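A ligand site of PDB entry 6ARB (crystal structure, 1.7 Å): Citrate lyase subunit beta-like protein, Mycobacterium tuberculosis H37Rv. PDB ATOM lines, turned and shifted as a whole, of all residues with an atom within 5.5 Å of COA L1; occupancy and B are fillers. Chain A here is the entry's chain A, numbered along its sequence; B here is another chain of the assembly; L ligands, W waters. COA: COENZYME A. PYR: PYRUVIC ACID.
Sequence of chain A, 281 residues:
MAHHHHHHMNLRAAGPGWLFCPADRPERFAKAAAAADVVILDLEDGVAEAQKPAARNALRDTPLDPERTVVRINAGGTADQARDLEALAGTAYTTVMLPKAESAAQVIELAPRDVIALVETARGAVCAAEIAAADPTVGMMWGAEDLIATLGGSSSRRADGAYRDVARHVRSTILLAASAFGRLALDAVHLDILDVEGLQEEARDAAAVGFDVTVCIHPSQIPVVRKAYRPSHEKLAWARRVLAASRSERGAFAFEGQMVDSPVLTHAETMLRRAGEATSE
Pro 22 touches COA L1 (CG to O9P, 3.4 Å). Arg 25 touches COA L1. Ala 32 touches COA L1. Asp 42 touches COA L1 (OD2 to C3P, 3.5 Å). Gly 46 touches COA L1 (N to C3P, 3.9 Å). Arg 72 touches COA L1 (NH2 to C2P, 3.2 Å). CD of Pro 219 touches C5A of COA L1 (3.4 Å). CB of Ala 252 of chain B touches C6P of COA L1 (3.5 Å). CA of Phe 253 of chain B touches CDP of COA L1, 3.9 Å away. Asp 261 of chain B touches COA L1. Hydrophobic or aromatic side chains within 4 Å of COA L1: Phe 20, Pro 22, Ala 32, Ile 217, His 218, Pro 219, Ala 252 of chain B and Met 259 of chain B. 16 residues have an atom within 4 Å of COA L1: Phe 20, Cys 21, Pro 22, Arg 25, Arg 28, Ala 32, Asp 42, Gly 46, Arg 72, Ile 217, His 218, Pro 219, Ala 252 of chain B, Phe 253 of chain B, Met 259 of chain B and Asp 261 of chain B.
Water W1 lies within hydrogen-bond range of OD2 of Asp 261 of chain B (2.6 Å), S1P of COA L1 (3.0 Å) and NH2 of Arg 72 (3.2 Å).
The guanidinium group (NE) of Arg 72 lies within salt-bridge range of the side-chain carboxylate (OD1) of Asp 42, at 2.8 Å. The backbone NH (N) of Ala 252 of chain B sits at hydrogen-bond distance from the backbone carbonyl oxygen (O) of Gly 46 (2.9 Å). O of Leu 191 sits at hydrogen-bond distance from N of Met 259 of chain B. The backbone carbonyl oxygen of Cys 21 lies within hydrogen-bond range of the backbone NH of Asp 42, at 3.0 Å. N of Gly 46 is in hydrogen-bond range of OD2 of Asp 42.
The side-chain sulfur of Met 259 of chain B lies close to a nitrogen (N4P) of COA L1 (3.7 Å). SG of Cys 21 is in hydrogen-bond range of N1A of COA L1, at 3.4 Å. The backbone carbonyl oxygen (O) of Ile 217 is in hydrogen-bond range of a nitrogen (N8P) of COA L1 (2.9 Å). O of Phe 20 lies within hydrogen-bond range of N6A of COA L1, at 2.9 Å. A ring nitrogen (NE2) of His 218 is in hydrogen-bond range of an oxygen (O2A) of COA L1 (2.6 Å). O3 of PYR L2 sits close to NH1 of Arg 72 (3.0 Å). The guanidinium group (NH2) of Arg 28 is in salt-bridge range of an oxygen (O5A) of COA L1 (2.9 Å).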
ATOM      1  N   LEU A  19       9.585  -8.437 -24.694  1.00  0.00           N
ATOM      2  CA  LEU A  19       8.361  -8.225 -25.460  1.00  0.00           C
ATOM      3  C   LEU A  19       7.595  -6.992 -25.020  1.00  0.00           C
ATOM      4  O   LEU A  19       7.262  -6.862 -23.850  1.00  0.00           O
ATOM      5  CB  LEU A  19       7.442  -9.459 -25.338  1.00  0.00           C
ATOM      6  CG  LEU A  19       6.033  -9.436 -25.933  1.00  0.00           C
ATOM      7  CD1 LEU A  19       6.071  -9.176 -27.444  1.00  0.00           C
ATOM      8  CD2 LEU A  19       5.365 -10.779 -25.646  1.00  0.00           C
ATOM      9  N   PHE A  20       7.346  -6.089 -25.968  1.00  0.00           N
ATOM     10  CA  PHE A  20       6.450  -4.954 -25.761  1.00  0.00           C
ATOM     11  C   PHE A  20       4.990  -5.427 -25.638  1.00  0.00           C
ATOM     12  O   PHE A  20       4.515  -6.215 -26.442  1.00  0.00           O
ATOM     13  CB  PHE A  20       6.511  -3.999 -26.959  1.00  0.00           C
ATOM     14  CG  PHE A  20       7.567  -2.929 -26.859  1.00  0.00           C
ATOM     15  CD1 PHE A  20       7.467  -1.930 -25.900  1.00  0.00           C
ATOM     16  CD2 PHE A  20       8.619  -2.883 -27.763  1.00  0.00           C
ATOM     17  CE1 PHE A  20       8.430  -0.930 -25.821  1.00  0.00           C
ATOM     18  CE2 PHE A  20       9.571  -1.888 -27.690  1.00  0.00           C
ATOM     19  CZ  PHE A  20       9.482  -0.904 -26.720  1.00  0.00           C
ATOM     20  N   CYS A  21       4.270  -4.889 -24.658  1.00  0.00           N
ATOM     21  CA  CYS A  21       2.815  -5.038 -24.638  1.00  0.00           C
ATOM     22  C   CYS A  21       2.188  -3.718 -24.208  1.00  0.00           C
ATOM     23  O   CYS A  21       2.568  -3.165 -23.174  1.00  0.00           O
ATOM     24  CB  CYS A  21       2.399  -6.190 -23.726  1.00  0.00           C
ATOM     25  SG  CYS A  21       0.613  -6.542 -23.687  1.00  0.00           S
ATOM     26  N   PRO A  22       1.249  -3.190 -25.014  1.00  0.00           N
ATOM     27  CA  PRO A  22       0.548  -1.936 -24.709  1.00  0.00           C
ATOM     28  C   PRO A  22      -0.150  -1.985 -23.351  1.00  0.00           C
ATOM     29  O   PRO A  22      -0.863  -2.948 -23.038  1.00  0.00           O
ATOM     30  CB  PRO A  22      -0.502  -1.846 -25.816  1.00  0.00           C
ATOM     31  CG  PRO A  22       0.103  -2.586 -26.966  1.00  0.00           C
ATOM     32  CD  PRO A  22       0.920  -3.699 -26.352  1.00  0.00           C
ATOM     33  N   ARG A  25      -3.947  -2.883 -22.614  1.00  0.00           N
ATOM     34  CA  ARG A  25      -4.414  -4.232 -22.963  1.00  0.00           C
ATOM     35  C   ARG A  25      -4.036  -5.217 -21.866  1.00  0.00           C
ATOM     36  O   ARG A  25      -3.285  -6.166 -22.104  1.00  0.00           O
ATOM     37  CB  ARG A  25      -3.812  -4.665 -24.295  1.00  0.00           C
ATOM     38  CG  ARG A  25      -4.039  -3.671 -25.416  1.00  0.00           C
ATOM     39  CD  ARG A  25      -4.908  -4.260 -26.509  1.00  0.00           C
ATOM     40  NE  ARG A  25      -4.516  -3.778 -27.842  1.00  0.00           N
ATOM     41  CZ  ARG A  25      -5.071  -4.196 -28.975  1.00  0.00           C
ATOM     42  NH1 ARG A  25      -6.044  -5.109 -28.938  1.00  0.00           N
ATOM     43  NH2 ARG A  25      -4.662  -3.716 -30.130  1.00  0.00           N
ATOM     44  N   ARG A  28      -3.768  -9.153 -21.835  1.00  0.00           N
ATOM     45  CA  ARG A  28      -2.629  -9.779 -22.496  1.00  0.00           C
ATOM     46  C   ARG A  28      -1.377  -9.770 -21.635  1.00  0.00           C
ATOM     47  O   ARG A  28      -0.367 -10.376 -21.999  1.00  0.00           O
ATOM     48  CB  ARG A  28      -2.328  -9.068 -23.817  1.00  0.00           C
ATOM     49  CG  ARG A  28      -3.428  -9.156 -24.845  1.00  0.00           C
ATOM     50  CD  ARG A  28      -3.026  -8.442 -26.129  1.00  0.00           C
ATOM     51  NE  ARG A  28      -4.117  -8.439 -27.102  1.00  0.00           N
ATOM     52  CZ  ARG A  28      -3.967  -8.142 -28.389  1.00  0.00           C
ATOM     53  NH1 ARG A  28      -2.758  -7.838 -28.854  1.00  0.00           N
ATOM     54  NH2 ARG A  28      -5.005  -8.166 -29.201  1.00  0.00           N
ATOM     55  N   LYS A  31      -0.235 -13.203 -20.503  1.00  0.00           N
ATOM     56  CA  LYS A  31       0.219 -13.906 -21.699  1.00  0.00           C
ATOM     57  C   LYS A  31       1.614 -13.430 -22.083  1.00  0.00           C
ATOM     58  O   LYS A  31       2.514 -14.230 -22.306  1.00  0.00           O
ATOM     59  CB  LYS A  31      -0.760 -13.685 -22.863  1.00  0.00           C
ATOM     60  CG  LYS A  31      -0.366 -14.400 -24.140  1.00  0.00           C
ATOM     61  CD  LYS A  31      -0.230 -15.893 -23.922  1.00  0.00           C
ATOM     62  CE  LYS A  31       0.249 -16.602 -25.188  1.00  0.00           C
ATOM     63  NZ  LYS A  31       0.339 -18.076 -25.002  1.00  0.00           N
ATOM     64  N   ALA A  32       1.792 -12.122 -22.154  1.00  0.00           N
ATOM     65  CA  ALA A  32       3.090 -11.529 -22.410  1.00  0.00           C
ATOM     66  C   ALA A  32       4.133 -12.080 -21.446  1.00  0.00           C
ATOM     67  O   ALA A  32       5.181 -12.581 -21.863  1.00  0.00           O
ATOM     68  CB  ALA A  32       2.999 -10.011 -22.288  1.00  0.00           C
ATOM     69  N   ASP A  42       3.918  -0.722 -22.102  1.00  0.00           N
ATOM     70  CA  ASP A  42       4.084   0.538 -22.832  1.00  0.00           C
ATOM     71  C   ASP A  42       3.009   1.594 -22.570  1.00  0.00           C
ATOM     72  O   ASP A  42       1.831   1.359 -22.802  1.00  0.00           O
ATOM     73  CB  ASP A  42       4.159   0.268 -24.341  1.00  0.00           C
ATOM     74  CG  ASP A  42       4.515   1.506 -25.134  1.00  0.00           C
ATOM     75  OD1 ASP A  42       5.154   2.417 -24.573  1.00  0.00           O
ATOM     76  OD2 ASP A  42       4.160   1.569 -26.337  1.00  0.00           O
ATOM     77  N   ASP A  45       4.062   5.170 -27.358  1.00  0.00           N
ATOM     78  CA  ASP A  45       3.443   5.093 -28.688  1.00  0.00           C
ATOM     79  C   ASP A  45       2.496   3.914 -28.955  1.00  0.00           C
ATOM     80  O   ASP A  45       1.686   3.973 -29.882  1.00  0.00           O
ATOM     81  CB  ASP A  45       4.490   5.227 -29.795  1.00  0.00           C
ATOM     82  CG  ASP A  45       5.083   6.625 -29.875  1.00  0.00           C
ATOM     83  OD1 ASP A  45       4.518   7.546 -29.236  1.00  0.00           O
ATOM     84  OD2 ASP A  45       6.087   6.824 -30.586  1.00  0.00           O
ATOM     85  N   GLY A  46       2.584   2.841 -28.164  1.00  0.00           N
ATOM     86  CA  GLY A  46       1.675   1.710 -28.320  1.00  0.00           C
ATOM     87  C   GLY A  46       0.241   2.072 -27.970  1.00  0.00           C
ATOM     88  O   GLY A  46      -0.729   1.390 -28.352  1.00  0.00           O
ATOM     89  N   ARG A  72       7.753   1.355 -20.254  1.00  0.00           N
ATOM     90  CA  ARG A  72       8.148   2.477 -21.106  1.00  0.00           C
ATOM     91  C   ARG A  72       7.237   3.668 -20.848  1.00  0.00           C
ATOM     92  O   ARG A  72       6.035   3.629 -21.128  1.00  0.00           O
ATOM     93  CB  ARG A  72       8.158   2.121 -22.599  1.00  0.00           C
ATOM     94  CG  ARG A  72       8.660   3.297 -23.448  1.00  0.00           C
ATOM     95  CD  ARG A  72       8.946   2.913 -24.885  1.00  0.00           C
ATOM     96  NE  ARG A  72       7.721   2.777 -25.666  1.00  0.00           N
ATOM     97  CZ  ARG A  72       7.697   2.687 -26.991  1.00  0.00           C
ATOM     98  NH1 ARG A  72       8.834   2.709 -27.676  1.00  0.00           N
ATOM     99  NH2 ARG A  72       6.531   2.547 -27.632  1.00  0.00           N
ATOM    100  N   VAL A 189      13.203  -3.337 -32.678  1.00  0.00           N
ATOM    101  CA  VAL A 189      12.062  -4.227 -32.959  1.00  0.00           C
ATOM    102  C   VAL A 189      11.988  -4.611 -34.444  1.00  0.00           C
ATOM    103  O   VAL A 189      12.450  -3.871 -35.312  1.00  0.00           O
ATOM    104  CB  VAL A 189      10.729  -3.580 -32.539  1.00  0.00           C
ATOM    105  CG1 VAL A 189      10.719  -3.296 -31.021  1.00  0.00           C
ATOM    106  CG2 VAL A 189      10.483  -2.307 -33.327  1.00  0.00           C
ATOM    107  N   LEU A 191       9.329  -5.092 -37.139  1.00  0.00           N
ATOM    108  CA  LEU A 191       7.937  -4.704 -37.324  1.00  0.00           C
ATOM    109  C   LEU A 191       7.131  -5.649 -38.221  1.00  0.00           C
ATOM    110  O   LEU A 191       5.905  -5.694 -38.127  1.00  0.00           O
ATOM    111  CB  LEU A 191       7.841  -3.292 -37.896  1.00  0.00           C
ATOM    112  CG  LEU A 191       8.344  -2.154 -37.003  1.00  0.00           C
ATOM    113  CD1 LEU A 191       7.889  -0.835 -37.593  1.00  0.00           C
ATOM    114  CD2 LEU A 191       7.820  -2.322 -35.602  1.00  0.00           C
ATOM    115  N   ILE A 193       5.792  -8.781 -38.680  1.00  0.00           N
ATOM    116  CA  ILE A 193       5.496  -9.853 -37.723  1.00  0.00           C
ATOM    117  C   ILE A 193       5.761 -11.264 -38.228  1.00  0.00           C
ATOM    118  O   ILE A 193       6.359 -12.069 -37.513  1.00  0.00           O
ATOM    119  CB  ILE A 193       4.044  -9.765 -37.255  1.00  0.00           C
ATOM    120  CG1 ILE A 193       3.826  -8.501 -36.421  1.00  0.00           C
ATOM    121  CG2 ILE A 193       3.667 -11.015 -36.458  1.00  0.00           C
ATOM    122  CD1 ILE A 193       2.383  -8.020 -36.357  1.00  0.00           C
ATOM    123  N   ILE A 217       7.735  -7.455 -30.752  1.00  0.00           N
ATOM    124  CA  ILE A 217       6.411  -6.844 -30.662  1.00  0.00           C
ATOM    125  C   ILE A 217       5.247  -7.867 -30.802  1.00  0.00           C
ATOM    126  O   ILE A 217       4.086  -7.480 -30.817  1.00  0.00           O
ATOM    127  CB  ILE A 217       6.253  -5.643 -31.632  1.00  0.00           C
ATOM    128  CG1 ILE A 217       6.788  -5.968 -33.031  1.00  0.00           C
ATOM    129  CG2 ILE A 217       7.004  -4.414 -31.104  1.00  0.00           C
ATOM    130  CD1 ILE A 217       6.007  -7.036 -33.767  1.00  0.00           C
ATOM    131  N   HIS A 218       5.585  -9.153 -30.873  1.00  0.00           N
ATOM    132  CA  HIS A 218       4.582 -10.221 -30.962  1.00  0.00           C
ATOM    133  C   HIS A 218       5.158 -11.456 -30.277  1.00  0.00           C
ATOM    134  O   HIS A 218       6.338 -11.752 -30.447  1.00  0.00           O
ATOM    135  CB  HIS A 218       4.234 -10.531 -32.421  1.00  0.00           C
ATOM    136  CG  HIS A 218       2.988 -11.352 -32.596  1.00  0.00           C
ATOM    137  ND1 HIS A 218       2.975 -12.722 -32.447  1.00  0.00           N
ATOM    138  CD2 HIS A 218       1.730 -10.986 -32.911  1.00  0.00           C
ATOM    139  CE1 HIS A 218       1.744 -13.166 -32.652  1.00  0.00           C
ATOM    140  NE2 HIS A 218       0.970 -12.136 -32.940  1.00  0.00           N
ATOM    141  N   PRO A 219       4.347 -12.168 -29.471  1.00  0.00           N
ATOM    142  CA  PRO A 219       4.908 -13.292 -28.704  1.00  0.00           C
ATOM    143  C   PRO A 219       5.454 -14.400 -29.596  1.00  0.00           C
ATOM    144  O   PRO A 219       6.286 -15.172 -29.145  1.00  0.00           O
ATOM    145  CB  PRO A 219       3.708 -13.798 -27.877  1.00  0.00           C
ATOM    146  CG  PRO A 219       2.502 -13.209 -28.522  1.00  0.00           C
ATOM    147  CD  PRO A 219       2.935 -11.901 -29.124  1.00  0.00           C
ATOM    148  N   ALA B 252      -1.234   1.084 -31.212  1.00  0.00           N
ATOM    149  CA  ALA B 252      -0.584   0.159 -32.122  1.00  0.00           C
ATOM    150  C   ALA B 252      -1.579  -0.786 -32.755  1.00  0.00           C
ATOM    151  O   ALA B 252      -2.513  -1.239 -32.096  1.00  0.00           O
ATOM    152  CB  ALA B 252       0.490  -0.627 -31.396  1.00  0.00           C
ATOM    153  N   PHE B 253      -1.393  -1.054 -34.033  1.00  0.00           N
ATOM    154  CA  PHE B 253      -2.220  -2.035 -34.725  1.00  0.00           C
ATOM    155  C   PHE B 253      -1.428  -2.650 -35.863  1.00  0.00           C
ATOM    156  O   PHE B 253      -0.431  -2.092 -36.318  1.00  0.00           O
ATOM    157  CB  PHE B 253      -3.510  -1.400 -35.249  1.00  0.00           C
ATOM    158  CG  PHE B 253      -3.304  -0.405 -36.358  1.00  0.00           C
ATOM    159  CD1 PHE B 253      -3.513  -0.763 -37.676  1.00  0.00           C
ATOM    160  CD2 PHE B 253      -2.926   0.905 -36.073  1.00  0.00           C
ATOM    161  CE1 PHE B 253      -3.338   0.154 -38.705  1.00  0.00           C
ATOM    162  CE2 PHE B 253      -2.738   1.819 -37.090  1.00  0.00           C
ATOM    163  CZ  PHE B 253      -2.949   1.448 -38.408  1.00  0.00           C
ATOM    164  N   ALA B 254      -1.894  -3.802 -36.337  1.00  0.00           N
ATOM    165  CA  ALA B 254      -1.231  -4.485 -37.430  1.00  0.00           C
ATOM    166  C   ALA B 254      -1.896  -4.124 -38.759  1.00  0.00           C
ATOM    167  O   ALA B 254      -3.115  -4.231 -38.902  1.00  0.00           O
ATOM    168  CB  ALA B 254      -1.249  -5.979 -37.208  1.00  0.00           C
ATOM    169  N   MET B 259       3.565  -4.163 -37.875  1.00  0.00           N
ATOM    170  CA  MET B 259       3.185  -3.418 -36.686  1.00  0.00           C
ATOM    171  C   MET B 259       3.256  -1.938 -37.035  1.00  0.00           C
ATOM    172  O   MET B 259       4.275  -1.465 -37.544  1.00  0.00           O
ATOM    173  CB  MET B 259       4.126  -3.734 -35.520  1.00  0.00           C
ATOM    174  CG  MET B 259       3.535  -3.469 -34.120  1.00  0.00           C
ATOM    175  SD  MET B 259       3.509  -1.738 -33.630  1.00  0.00           S
ATOM    176  CE  MET B 259       5.254  -1.366 -33.537  1.00  0.00           C
ATOM    177  N   ASP B 261       2.559   2.041 -35.634  1.00  0.00           N
ATOM    178  CA  ASP B 261       2.201   3.027 -34.630  1.00  0.00           C
ATOM    179  C   ASP B 261       2.669   4.416 -35.053  1.00  0.00           C
ATOM    180  O   ASP B 261       2.970   4.630 -36.224  1.00  0.00           O
ATOM    181  CB  ASP B 261       2.702   2.628 -33.232  1.00  0.00           C
ATOM    182  CG  ASP B 261       4.207   2.730 -33.098  1.00  0.00           C
ATOM    183  OD1 ASP B 261       4.904   2.886 -34.124  1.00  0.00           O
ATOM    184  OD2 ASP B 261       4.693   2.649 -31.946  1.00  0.00           O
HETATM  185  N1A COA L   1       1.572  -8.937 -25.976  1.00  0.00           N
HETATM  186  C2A COA L   1       0.847  -9.962 -25.505  1.00  0.00           C
HETATM  187  N3A COA L   1       0.113 -10.740 -26.327  1.00  0.00           N
HETATM  188  C4A COA L   1       0.075 -10.509 -27.651  1.00  0.00           C
HETATM  189  C5A COA L   1       0.811  -9.439 -28.179  1.00  0.00           C
HETATM  190  C6A COA L   1       1.569  -8.660 -27.297  1.00  0.00           C
HETATM  191  N6A COA L   1       2.371  -7.525 -27.835  1.00  0.00           N
HETATM  192  N7A COA L   1       0.608  -9.426 -29.518  1.00  0.00           N
HETATM  193  C8A COA L   1      -0.232 -10.443 -29.826  1.00  0.00           C
HETATM  194  N9A COA L   1      -0.568 -11.086 -28.696  1.00  0.00           N
HETATM  195  C1B COA L   1      -1.424 -12.239 -28.597  1.00  0.00           C
HETATM  196  C2B COA L   1      -2.823 -11.988 -28.904  1.00  0.00           C
HETATM  197  O2B COA L   1      -3.477 -11.657 -27.727  1.00  0.00           O
HETATM  198  C3B COA L   1      -3.280 -13.271 -29.331  1.00  0.00           C
HETATM  199  O3B COA L   1      -3.432 -14.044 -28.204  1.00  0.00           O
HETATM  200  P3B COA L   1      -4.402 -15.253 -28.229  1.00  0.00           P
HETATM  201  O7A COA L   1      -5.013 -15.356 -29.606  1.00  0.00           O
HETATM  202  O8A COA L   1      -5.475 -15.026 -27.195  1.00  0.00           O
HETATM  203  O9A COA L   1      -3.631 -16.526 -27.912  1.00  0.00           O
HETATM  204  C4B COA L   1      -2.156 -13.798 -30.105  1.00  0.00           C
HETATM  205  O4B COA L   1      -0.993 -13.193 -29.514  1.00  0.00           O
HETATM  206  C5B COA L   1      -2.261 -13.429 -31.507  1.00  0.00           C
HETATM  207  O5B COA L   1      -2.706 -12.167 -31.784  1.00  0.00           O
HETATM  208  P1A COA L   1      -2.553 -11.482 -33.163  1.00  0.00           P
HETATM  209  O1A COA L   1      -3.842 -11.628 -33.901  1.00  0.00           O
HETATM  210  O2A COA L   1      -1.440 -12.122 -33.942  1.00  0.00           O
HETATM  211  O3A COA L   1      -2.223  -9.975 -32.891  1.00  0.00           O
HETATM  212  P2A COA L   1      -3.294  -8.814 -32.935  1.00  0.00           P
HETATM  213  O4A COA L   1      -3.960  -8.771 -34.291  1.00  0.00           O
HETATM  214  O5A COA L   1      -4.330  -8.997 -31.855  1.00  0.00           O
HETATM  215  O6A COA L   1      -2.594  -7.446 -32.699  1.00  0.00           O
HETATM  216  CBP COA L   1      -0.601  -6.039 -32.433  1.00  0.00           C
HETATM  217  CCP COA L   1      -1.273  -7.256 -33.078  1.00  0.00           C
HETATM  218  CDP COA L   1      -1.629  -4.959 -32.151  1.00  0.00           C
HETATM  219  CEP COA L   1       0.486  -5.484 -33.328  1.00  0.00           C
HETATM  220  CAP COA L   1       0.038  -6.546 -31.115  1.00  0.00           C
HETATM  221  OAP COA L   1       0.984  -7.495 -31.451  1.00  0.00           O
HETATM  222  C9P COA L   1       0.781  -5.484 -30.321  1.00  0.00           C
HETATM  223  O9P COA L   1       0.196  -4.797 -29.490  1.00  0.00           O
HETATM  224  N8P COA L   1       2.164  -5.319 -30.585  1.00  0.00           N
HETATM  225  C7P COA L   1       2.961  -4.316 -29.849  1.00  0.00           C
HETATM  226  C6P COA L   1       2.924  -2.898 -30.346  1.00  0.00           C
HETATM  227  C5P COA L   1       3.728  -1.950 -29.506  1.00  0.00           C
HETATM  228  O5P COA L   1       3.834  -2.161 -28.304  1.00  0.00           O
HETATM  229  N4P COA L   1       4.337  -0.808 -30.134  1.00  0.00           N
HETATM  230  C3P COA L   1       5.107   0.088 -29.334  1.00  0.00           C
HETATM  231  C2P COA L   1       6.585  -0.216 -29.307  1.00  0.00           C
HETATM  232  S1P COA L   1       7.296  -0.749 -30.856  1.00  0.00           S
HETATM  233  C   PYR L   2      10.911   3.132 -32.620  1.00  0.00           C
HETATM  234  O   PYR L   2      11.556   2.501 -33.576  1.00  0.00           O
HETATM  235  OXT PYR L   2      10.476   4.335 -32.874  1.00  0.00           O
HETATM  236  CA  PYR L   2      10.705   2.514 -31.371  1.00  0.00           C
HETATM  237  O3  PYR L   2       9.817   2.952 -30.514  1.00  0.00           O
HETATM  238  CB  PYR L   2      11.527   1.319 -30.988  1.00  0.00           C
HETATM  239  O   HOH W   1       7.001   2.245 -30.738  1.00  0.00           O
HETATM  240  O   HOH W   2      -6.419 -12.757 -28.954  1.00  0.00           O
